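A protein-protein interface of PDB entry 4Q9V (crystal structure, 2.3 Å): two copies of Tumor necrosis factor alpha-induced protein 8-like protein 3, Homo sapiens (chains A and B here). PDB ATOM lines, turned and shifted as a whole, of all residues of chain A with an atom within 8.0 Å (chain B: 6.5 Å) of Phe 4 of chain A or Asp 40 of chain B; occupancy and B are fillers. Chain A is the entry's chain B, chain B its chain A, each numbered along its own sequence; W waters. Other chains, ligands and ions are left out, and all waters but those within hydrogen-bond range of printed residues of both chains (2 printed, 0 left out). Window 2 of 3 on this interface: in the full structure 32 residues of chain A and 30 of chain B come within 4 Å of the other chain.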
ATOM      1  N   ALA A   1       8.474   7.238 -16.202  1.00  0.00           N
ATOM      2  CA  ALA A   1       9.261   6.994 -17.403  1.00  0.00           C
ATOM      3  C   ALA A   1       9.596   5.513 -17.549  1.00  0.00           C
ATOM      4  O   ALA A   1       9.364   4.917 -18.598  1.00  0.00           O
ATOM      5  CB  ALA A   1      10.533   7.825 -17.383  1.00  0.00           C
ATOM      6  N   MET A   2      10.144   4.929 -16.489  1.00  0.00           N
ATOM      7  CA  MET A   2      10.504   3.515 -16.496  1.00  0.00           C
ATOM      8  C   MET A   2       9.283   2.643 -16.775  1.00  0.00           C
ATOM      9  O   MET A   2       8.256   2.760 -16.110  1.00  0.00           O
ATOM     10  CB  MET A   2      11.144   3.121 -15.162  1.00  0.00           C
ATOM     11  CG  MET A   2      11.714   1.714 -15.129  1.00  0.00           C
ATOM     12  SD  MET A   2      12.712   1.323 -16.578  1.00  0.00           S
ATOM     13  CE  MET A   2      12.676  -0.467 -16.540  1.00  0.00           C
ATOM     14  N   VAL A   3       9.402   1.775 -17.771  1.00  0.00           N
ATOM     15  CA  VAL A   3       8.302   0.905 -18.161  1.00  0.00           C
ATOM     16  C   VAL A   3       8.314  -0.396 -17.368  1.00  0.00           C
ATOM     17  O   VAL A   3       9.225  -0.649 -16.582  1.00  0.00           O
ATOM     18  CB  VAL A   3       8.360   0.568 -19.660  1.00  0.00           C
ATOM     19  CG1 VAL A   3       8.469   1.842 -20.481  1.00  0.00           C
ATOM     20  CG2 VAL A   3       9.530  -0.358 -19.950  1.00  0.00           C
ATOM     21  N   PHE A   4       7.291  -1.215 -17.581  1.00  0.00           N
ATOM     22  CA  PHE A   4       7.212  -2.512 -16.936  1.00  0.00           C
ATOM     23  C   PHE A   4       8.387  -3.390 -17.335  1.00  0.00           C
ATOM     24  O   PHE A   4       8.769  -3.442 -18.520  1.00  0.00           O
ATOM     25  CB  PHE A   4       5.931  -3.223 -17.320  1.00  0.00           C
ATOM     26  CG  PHE A   4       5.848  -4.606 -16.771  1.00  0.00           C
ATOM     27  CD1 PHE A   4       5.388  -4.810 -15.484  1.00  0.00           C
ATOM     28  CD2 PHE A   4       6.289  -5.704 -17.521  1.00  0.00           C
ATOM     29  CE1 PHE A   4       5.327  -6.097 -14.943  1.00  0.00           C
ATOM     30  CE2 PHE A   4       6.238  -6.984 -16.994  1.00  0.00           C
ATOM     31  CZ  PHE A   4       5.747  -7.186 -15.702  1.00  0.00           C
ATOM     32  N   SER A   5       8.959  -4.065 -16.343  1.00  0.00           N
ATOM     33  CA  SER A   5      10.014  -5.032 -16.610  1.00  0.00           C
ATOM     34  C   SER A   5       9.909  -6.262 -15.705  1.00  0.00           C
ATOM     35  O   SER A   5       9.884  -6.144 -14.489  1.00  0.00           O
ATOM     36  CB  SER A   5      11.384  -4.378 -16.479  1.00  0.00           C
ATOM     37  OG  SER A   5      12.391  -5.355 -16.596  1.00  0.00           O
ATOM     38  N   SER A   6       9.832  -7.436 -16.320  1.00  0.00           N
ATOM     39  CA  SER A   6       9.730  -8.679 -15.570  1.00  0.00           C
ATOM     40  C   SER A   6      11.021  -8.945 -14.812  1.00  0.00           C
ATOM     41  O   SER A   6      11.005  -9.493 -13.714  1.00  0.00           O
ATOM     42  CB  SER A   6       9.405  -9.851 -16.500  1.00  0.00           C
ATOM     43  OG  SER A   6      10.340  -9.942 -17.557  1.00  0.00           O
ATOM     44  N   LYS A   7      12.135  -8.541 -15.410  1.00  0.00           N
ATOM     45  CA  LYS A   7      13.437  -8.657 -14.777  1.00  0.00           C
ATOM     46  C   LYS A   7      13.424  -7.929 -13.440  1.00  0.00           C
ATOM     47  O   LYS A   7      13.925  -8.436 -12.441  1.00  0.00           O
ATOM     48  CB  LYS A   7      14.519  -8.062 -15.679  1.00  0.00           C
ATOM     49  CG  LYS A   7      15.409  -9.091 -16.351  1.00  0.00           C
ATOM     50  CD  LYS A   7      15.293  -9.015 -17.862  1.00  0.00           C
ATOM     51  CE  LYS A   7      16.119  -7.872 -18.429  1.00  0.00           C
ATOM     52  NZ  LYS A   7      15.518  -7.325 -19.677  1.00  0.00           N
ATOM     53  N   SER A   8      12.841  -6.735 -13.440  1.00  0.00           N
ATOM     54  CA  SER A   8      12.742  -5.925 -12.232  1.00  0.00           C
ATOM     55  C   SER A   8      11.969  -6.659 -11.147  1.00  0.00           C
ATOM     56  O   SER A   8      12.404  -6.720 -10.000  1.00  0.00           O
ATOM     57  CB  SER A   8      12.070  -4.583 -12.534  1.00  0.00           C
ATOM     58  OG  SER A   8      12.787  -3.861 -13.517  1.00  0.00           O
ATOM     59  N   LEU A   9      10.821  -7.219 -11.514  1.00  0.00           N
ATOM     60  CA  LEU A   9       9.999  -7.961 -10.553  1.00  0.00           C
ATOM     61  C   LEU A   9      10.778  -9.143  -9.980  1.00  0.00           C
ATOM     62  O   LEU A   9      10.786  -9.371  -8.767  1.00  0.00           O
ATOM     63  CB  LEU A   9       8.688  -8.442 -11.179  1.00  0.00           C
ATOM     64  CG  LEU A   9       7.487  -7.495 -11.208  1.00  0.00           C
ATOM     65  CD1 LEU A   9       7.832  -6.188 -11.909  1.00  0.00           C
ATOM     66  CD2 LEU A   9       6.272  -8.145 -11.886  1.00  0.00           C
ATOM     67  N   ALA A  10      11.450  -9.878 -10.863  1.00  0.00           N
ATOM     68  CA  ALA A  10      12.277 -11.017 -10.456  1.00  0.00           C
ATOM     69  C   ALA A  10      13.360 -10.611  -9.456  1.00  0.00           C
ATOM     70  O   ALA A  10      13.546 -11.292  -8.429  1.00  0.00           O
ATOM     71  CB  ALA A  10      12.895 -11.691 -11.664  1.00  0.00           C
ATOM     72  N   SER B  35      13.163 -15.273 -22.173  1.00  0.00           N
ATOM     73  CA  SER B  35      12.101 -15.489 -21.199  1.00  0.00           C
ATOM     74  C   SER B  35      11.515 -14.179 -20.687  1.00  0.00           C
ATOM     75  O   SER B  35      10.300 -14.013 -20.635  1.00  0.00           O
ATOM     76  CB  SER B  35      12.612 -16.329 -20.028  1.00  0.00           C
ATOM     77  OG  SER B  35      13.154 -17.556 -20.483  1.00  0.00           O
ATOM     78  N   SER B  36      12.385 -13.250 -20.305  1.00  0.00           N
ATOM     79  CA  SER B  36      11.942 -11.964 -19.783  1.00  0.00           C
ATOM     80  C   SER B  36      11.164 -11.176 -20.831  1.00  0.00           C
ATOM     81  O   SER B  36      10.261 -10.413 -20.497  1.00  0.00           O
ATOM     82  CB  SER B  36      13.129 -11.151 -19.263  1.00  0.00           C
ATOM     83  OG  SER B  36      13.674 -10.332 -20.279  1.00  0.00           O
ATOM     84  N   GLU B  37      11.516 -11.366 -22.097  1.00  0.00           N
ATOM     85  CA  GLU B  37      10.823 -10.690 -23.186  1.00  0.00           C
ATOM     86  C   GLU B  37       9.418 -11.254 -23.372  1.00  0.00           C
ATOM     87  O   GLU B  37       8.480 -10.519 -23.671  1.00  0.00           O
ATOM     88  CB  GLU B  37      11.620 -10.800 -24.487  1.00  0.00           C
ATOM     89  CG  GLU B  37      12.786  -9.829 -24.587  1.00  0.00           C
ATOM     90  CD  GLU B  37      12.336  -8.401 -24.830  1.00  0.00           C
ATOM     91  OE1 GLU B  37      13.128  -7.473 -24.557  1.00  0.00           O
ATOM     92  OE2 GLU B  37      11.194  -8.201 -25.292  1.00  0.00           O
ATOM     93  N   ILE B  38       9.278 -12.561 -23.193  1.00  0.00           N
ATOM     94  CA  ILE B  38       7.980 -13.212 -23.290  1.00  0.00           C
ATOM     95  C   ILE B  38       7.055 -12.684 -22.198  1.00  0.00           C
ATOM     96  O   ILE B  38       5.918 -12.311 -22.463  1.00  0.00           O
ATOM     97  CB  ILE B  38       8.101 -14.745 -23.178  1.00  0.00           C
ATOM     98  CG1 ILE B  38       8.839 -15.310 -24.391  1.00  0.00           C
ATOM     99  CG2 ILE B  38       6.731 -15.390 -23.047  1.00  0.00           C
ATOM    100  CD1 ILE B  38       9.126 -16.791 -24.295  1.00  0.00           C
ATOM    101  N   PHE B  39       7.561 -12.654 -20.971  1.00  0.00           N
ATOM    102  CA  PHE B  39       6.787 -12.169 -19.837  1.00  0.00           C
ATOM    103  C   PHE B  39       6.431 -10.696 -20.006  1.00  0.00           C
ATOM    104  O   PHE B  39       5.350 -10.265 -19.613  1.00  0.00           O
ATOM    105  CB  PHE B  39       7.554 -12.384 -18.533  1.00  0.00           C
ATOM    106  CG  PHE B  39       7.448 -13.779 -17.992  1.00  0.00           C
ATOM    107  CD1 PHE B  39       7.218 -14.850 -18.838  1.00  0.00           C
ATOM    108  CD2 PHE B  39       7.575 -14.020 -16.637  1.00  0.00           C
ATOM    109  CE1 PHE B  39       7.117 -16.134 -18.343  1.00  0.00           C
ATOM    110  CE2 PHE B  39       7.475 -15.304 -16.136  1.00  0.00           C
ATOM    111  CZ  PHE B  39       7.246 -16.363 -16.991  1.00  0.00           C
ATOM    112  N   ASP B  40       7.343  -9.930 -20.592  1.00  0.00           N
ATOM    113  CA  ASP B  40       7.106  -8.514 -20.842  1.00  0.00           C
ATOM    114  C   ASP B  40       5.972  -8.343 -21.844  1.00  0.00           C
ATOM    115  O   ASP B  40       5.074  -7.530 -21.641  1.00  0.00           O
ATOM    116  CB  ASP B  40       8.375  -7.832 -21.346  1.00  0.00           C
ATOM    117  CG  ASP B  40       9.343  -7.508 -20.231  1.00  0.00           C
ATOM    118  OD1 ASP B  40       8.992  -7.737 -19.058  1.00  0.00           O
ATOM    119  OD2 ASP B  40      10.457  -7.033 -20.523  1.00  0.00           O
ATOM    120  N   GLU B  41       6.015  -9.117 -22.921  1.00  0.00           N
ATOM    121  CA  GLU B  41       4.891  -9.155 -23.875  1.00  0.00           C
ATOM    122  C   GLU B  41       3.563  -9.593 -23.228  1.00  0.00           C
ATOM    123  O   GLU B  41       2.491  -9.065 -23.569  1.00  0.00           O
ATOM    124  CB  GLU B  41       5.166 -10.059 -25.074  1.00  0.00           C
ATOM    125  CG  GLU B  41       6.341  -9.700 -25.985  1.00  0.00           C
ATOM    126  CD  GLU B  41       6.313  -8.286 -26.512  1.00  0.00           C
ATOM    127  OE1 GLU B  41       5.225  -7.665 -26.555  1.00  0.00           O
ATOM    128  OE2 GLU B  41       7.396  -7.799 -26.901  1.00  0.00           O
ATOM    129  N   LEU B  42       3.620 -10.563 -22.318  1.00  0.00           N
ATOM    130  CA  LEU B  42       2.395 -11.056 -21.687  1.00  0.00           C
ATOM    131  C   LEU B  42       1.806  -9.912 -20.897  1.00  0.00           C
ATOM    132  O   LEU B  42       0.605  -9.704 -20.899  1.00  0.00           O
ATOM    133  CB  LEU B  42       2.665 -12.282 -20.784  1.00  0.00           C
ATOM    134  CG  LEU B  42       3.056 -13.552 -21.563  1.00  0.00           C
ATOM    135  CD1 LEU B  42       3.368 -14.717 -20.637  1.00  0.00           C
ATOM    136  CD2 LEU B  42       1.955 -13.939 -22.551  1.00  0.00           C
ATOM    137  N   TYR B  43       2.674  -9.134 -20.261  1.00  0.00           N
ATOM    138  CA  TYR B  43       2.237  -7.946 -19.542  1.00  0.00           C
ATOM    139  C   TYR B  43       1.516  -7.031 -20.497  1.00  0.00           C
ATOM    140  O   TYR B  43       0.401  -6.578 -20.222  1.00  0.00           O
ATOM    141  CB  TYR B  43       3.429  -7.188 -18.972  1.00  0.00           C
ATOM    142  CG  TYR B  43       3.048  -5.828 -18.441  1.00  0.00           C
ATOM    143  CD1 TYR B  43       2.379  -5.707 -17.238  1.00  0.00           C
ATOM    144  CD2 TYR B  43       3.342  -4.663 -19.152  1.00  0.00           C
ATOM    145  CE1 TYR B  43       2.029  -4.458 -16.718  1.00  0.00           C
ATOM    146  CE2 TYR B  43       2.980  -3.409 -18.645  1.00  0.00           C
ATOM    147  CZ  TYR B  43       2.325  -3.324 -17.431  1.00  0.00           C
ATOM    148  OH  TYR B  43       1.953  -2.113 -16.916  1.00  0.00           O
ATOM    149  N   LYS B  44       2.164  -6.753 -21.625  1.00  0.00           N
ATOM    150  CA  LYS B  44       1.600  -5.772 -22.562  1.00  0.00           C
ATOM    151  C   LYS B  44       0.206  -6.189 -23.020  1.00  0.00           C
ATOM    152  O   LYS B  44      -0.735  -5.384 -23.017  1.00  0.00           O
ATOM    153  CB  LYS B  44       2.553  -5.511 -23.737  1.00  0.00           C
ATOM    154  CG  LYS B  44       3.841  -4.749 -23.315  1.00  0.00           C
ATOM    155  CD  LYS B  44       4.786  -4.477 -24.507  1.00  0.00           C
ATOM    156  CE  LYS B  44       6.163  -4.052 -24.008  1.00  0.00           C
ATOM    157  NZ  LYS B  44       7.182  -3.967 -25.090  1.00  0.00           N
ATOM    158  N   VAL B  45       0.061  -7.467 -23.354  1.00  0.00           N
ATOM    159  CA  VAL B  45      -1.236  -7.985 -23.781  1.00  0.00           C
ATOM    160  C   VAL B  45      -2.300  -7.973 -22.672  1.00  0.00           C
ATOM    161  O   VAL B  45      -3.474  -7.663 -22.945  1.00  0.00           O
ATOM    162  CB  VAL B  45      -1.091  -9.377 -24.425  1.00  0.00           C
ATOM    163  CG1 VAL B  45      -2.442  -9.998 -24.642  1.00  0.00           C
ATOM    164  CG2 VAL B  45      -0.378  -9.234 -25.740  1.00  0.00           C
ATOM    165  N   LYS B  53      -3.474  -1.114 -15.803  1.00  0.00           N
ATOM    166  CA  LYS B  53      -2.031  -1.206 -15.608  1.00  0.00           C
ATOM    167  C   LYS B  53      -1.680  -1.956 -14.328  1.00  0.00           C
ATOM    168  O   LYS B  53      -0.958  -2.960 -14.353  1.00  0.00           O
ATOM    169  CB  LYS B  53      -1.459   0.214 -15.579  1.00  0.00           C
ATOM    170  CG  LYS B  53       0.029   0.344 -15.347  1.00  0.00           C
ATOM    171  CD  LYS B  53       0.492   1.723 -15.818  1.00  0.00           C
ATOM    172  CE  LYS B  53       1.995   1.914 -15.669  1.00  0.00           C
ATOM    173  NZ  LYS B  53       2.448   3.174 -16.333  1.00  0.00           N
ATOM    174  N   ALA B  56      -2.612  -5.697 -14.351  1.00  0.00           N
ATOM    175  CA  ALA B  56      -1.610  -6.370 -15.172  1.00  0.00           C
ATOM    176  C   ALA B  56      -0.359  -6.632 -14.345  1.00  0.00           C
ATOM    177  O   ALA B  56       0.148  -7.758 -14.313  1.00  0.00           O
ATOM    178  CB  ALA B  56      -1.273  -5.543 -16.370  1.00  0.00           C
ATOM    179  N   HIS B  57       0.101  -5.587 -13.658  1.00  0.00           N
ATOM    180  CA  HIS B  57       1.300  -5.662 -12.851  1.00  0.00           C
ATOM    181  C   HIS B  57       1.128  -6.746 -11.798  1.00  0.00           C
ATOM    182  O   HIS B  57       2.019  -7.551 -11.610  1.00  0.00           O
ATOM    183  CB  HIS B  57       1.626  -4.298 -12.203  1.00  0.00           C
ATOM    184  CG  HIS B  57       2.931  -4.270 -11.462  1.00  0.00           C
ATOM    185  ND1 HIS B  57       3.091  -4.818 -10.203  1.00  0.00           N
ATOM    186  CD2 HIS B  57       4.142  -3.764 -11.804  1.00  0.00           C
ATOM    187  CE1 HIS B  57       4.340  -4.651  -9.804  1.00  0.00           C
ATOM    188  NE2 HIS B  57       5.002  -4.017 -10.760  1.00  0.00           N
ATOM    189  N   MET B  60       1.280 -10.316 -13.435  1.00  0.00           N
ATOM    190  CA  MET B  60       2.672 -10.684 -13.750  1.00  0.00           C
ATOM    191  C   MET B  60       3.510 -10.945 -12.499  1.00  0.00           C
ATOM    192  O   MET B  60       4.326 -11.870 -12.454  1.00  0.00           O
ATOM    193  CB  MET B  60       3.334  -9.636 -14.640  1.00  0.00           C
ATOM    194  CG  MET B  60       2.666  -9.524 -15.993  1.00  0.00           C
ATOM    195  SD  MET B  60       2.438 -11.148 -16.764  1.00  0.00           S
ATOM    196  CE  MET B  60       4.170 -11.579 -17.084  1.00  0.00           C
ATOM    197  N   LYS B  61       3.274 -10.149 -11.467  1.00  0.00           N
ATOM    198  CA  LYS B  61       3.958 -10.326 -10.208  1.00  0.00           C
ATOM    199  C   LYS B  61       3.651 -11.677  -9.581  1.00  0.00           C
ATOM    200  O   LYS B  61       4.571 -12.338  -9.133  1.00  0.00           O
ATOM    201  CB  LYS B  61       3.631  -9.185  -9.226  1.00  0.00           C
ATOM    202  CG  LYS B  61       4.337  -9.352  -7.867  1.00  0.00           C
ATOM    203  CD  LYS B  61       4.166  -8.117  -6.970  1.00  0.00           C
ATOM    204  CE  LYS B  61       5.087  -8.182  -5.743  1.00  0.00           C
ATOM    205  NZ  LYS B  61       4.878  -7.039  -4.791  1.00  0.00           N
ATOM    206  N   ILE B  64       5.419 -14.409 -11.662  1.00  0.00           N
ATOM    207  CA  ILE B  64       6.840 -14.442 -11.365  1.00  0.00           C
ATOM    208  C   ILE B  64       7.139 -15.002  -9.993  1.00  0.00           C
ATOM    209  O   ILE B  64       8.102 -15.775  -9.824  1.00  0.00           O
ATOM    210  CB  ILE B  64       7.430 -13.012 -11.568  1.00  0.00           C
ATOM    211  CG1 ILE B  64       7.449 -12.705 -13.070  1.00  0.00           C
ATOM    212  CG2 ILE B  64       8.793 -12.873 -10.921  1.00  0.00           C
ATOM    213  CD1 ILE B  64       7.655 -11.258 -13.387  1.00  0.00           C
HETATM  214  O   HOH W   1      12.462  -6.957 -18.587  1.00  0.00           O
HETATM  215  O   HOH W   2      14.863  -7.431 -22.493  1.00  0.00           O
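The backbone carbonyl oxygen of Ser 36 of chain B lies within hydrogen-bond range of the side-chain hydroxyl of Ser 6 of chain A. The side-chain carboxylate (OD1) of Asp 40 of chain B is in hydrogen-bond range of the backbone NH (N) of Ser 6 of chain A (2.9 Å).
The backbone NH (N) of Lys 7 of chain A sits close to the side-chain hydroxyl (OG) of Ser 5 of chain A (3.4 Å). The side-chain hydroxyl (OG) of Ser 5 of chain A lies close to the side-chain hydroxyl (OG) of Ser 8 of chain A (3.4 Å).
Among the printed residues, pairs that only touch across the chains: Phe 4 of chain A with Asp 40 of chain B, Phe 4 of chain A with Tyr 43 of chain B, Phe 4 of chain A with Met 60 of chain B, Ser 5 of chain A with Asp 40 of chain B, Ser 6 of chain A with Phe 39 of chain B, Ser 6 of chain A with Ile 64 of chain B, Lys 7 of chain A with Ser 36 of chain B, Leu 9 of chain A with His 57 of chain B, Leu 9 of chain A with Met 60 of chain B, Leu 9 of chain A with Lys 61 of chain B, Leu 9 of chain A with Ile 64 of chain B and Ala 10 of chain A with Ile 64 of chain B.
Phe 4 of chain A touches just these residues of chain B: Asp 40, Tyr 43 and Met 60. Printed residues of chain A within 4 Å of Asp 40 of chain B: Phe 4 (3.5 Å), Ser 5 (3.8 Å) and Ser 6 (2.9 Å). Of the printed residues of chain B, Leu 9 of chain A touches His 57, Met 60, Lys 61 and Ile 64. Of the printed residues of chain A, His 57 of chain B touches Leu 9 (3.7 Å). The nearest residue of chain A that does not touch Asp 40 of chain B is Lys 7 of chain A (4.9 Å). The nearest printed residue of chain A that does not touch Tyr 43 of chain B is Val 3 of chain A (6.3 Å).
Hydrophobic or aromatic side chains of chain A that line the printed part of chain B: Phe 4 and Leu 9. Among the printed residues, no Asp or Glu carboxylate lies within 4 Å of a Lys or Arg side-chain nitrogen of the other chain.
No position is printed for both chains.
Water W1 lies within hydrogen-bond range of the side-chain hydroxyl of Ser 5 of chain A (2.6 Å), the side-chain carboxylate of Asp 40 of chain B (2.8 Å) and the side-chain amino group of Lys 7 of chain A (3.3 Å). Water W2 lies within hydrogen-bond range of OE1 of Glu 37 of chain B and NZ of Lys 7 of chain A.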
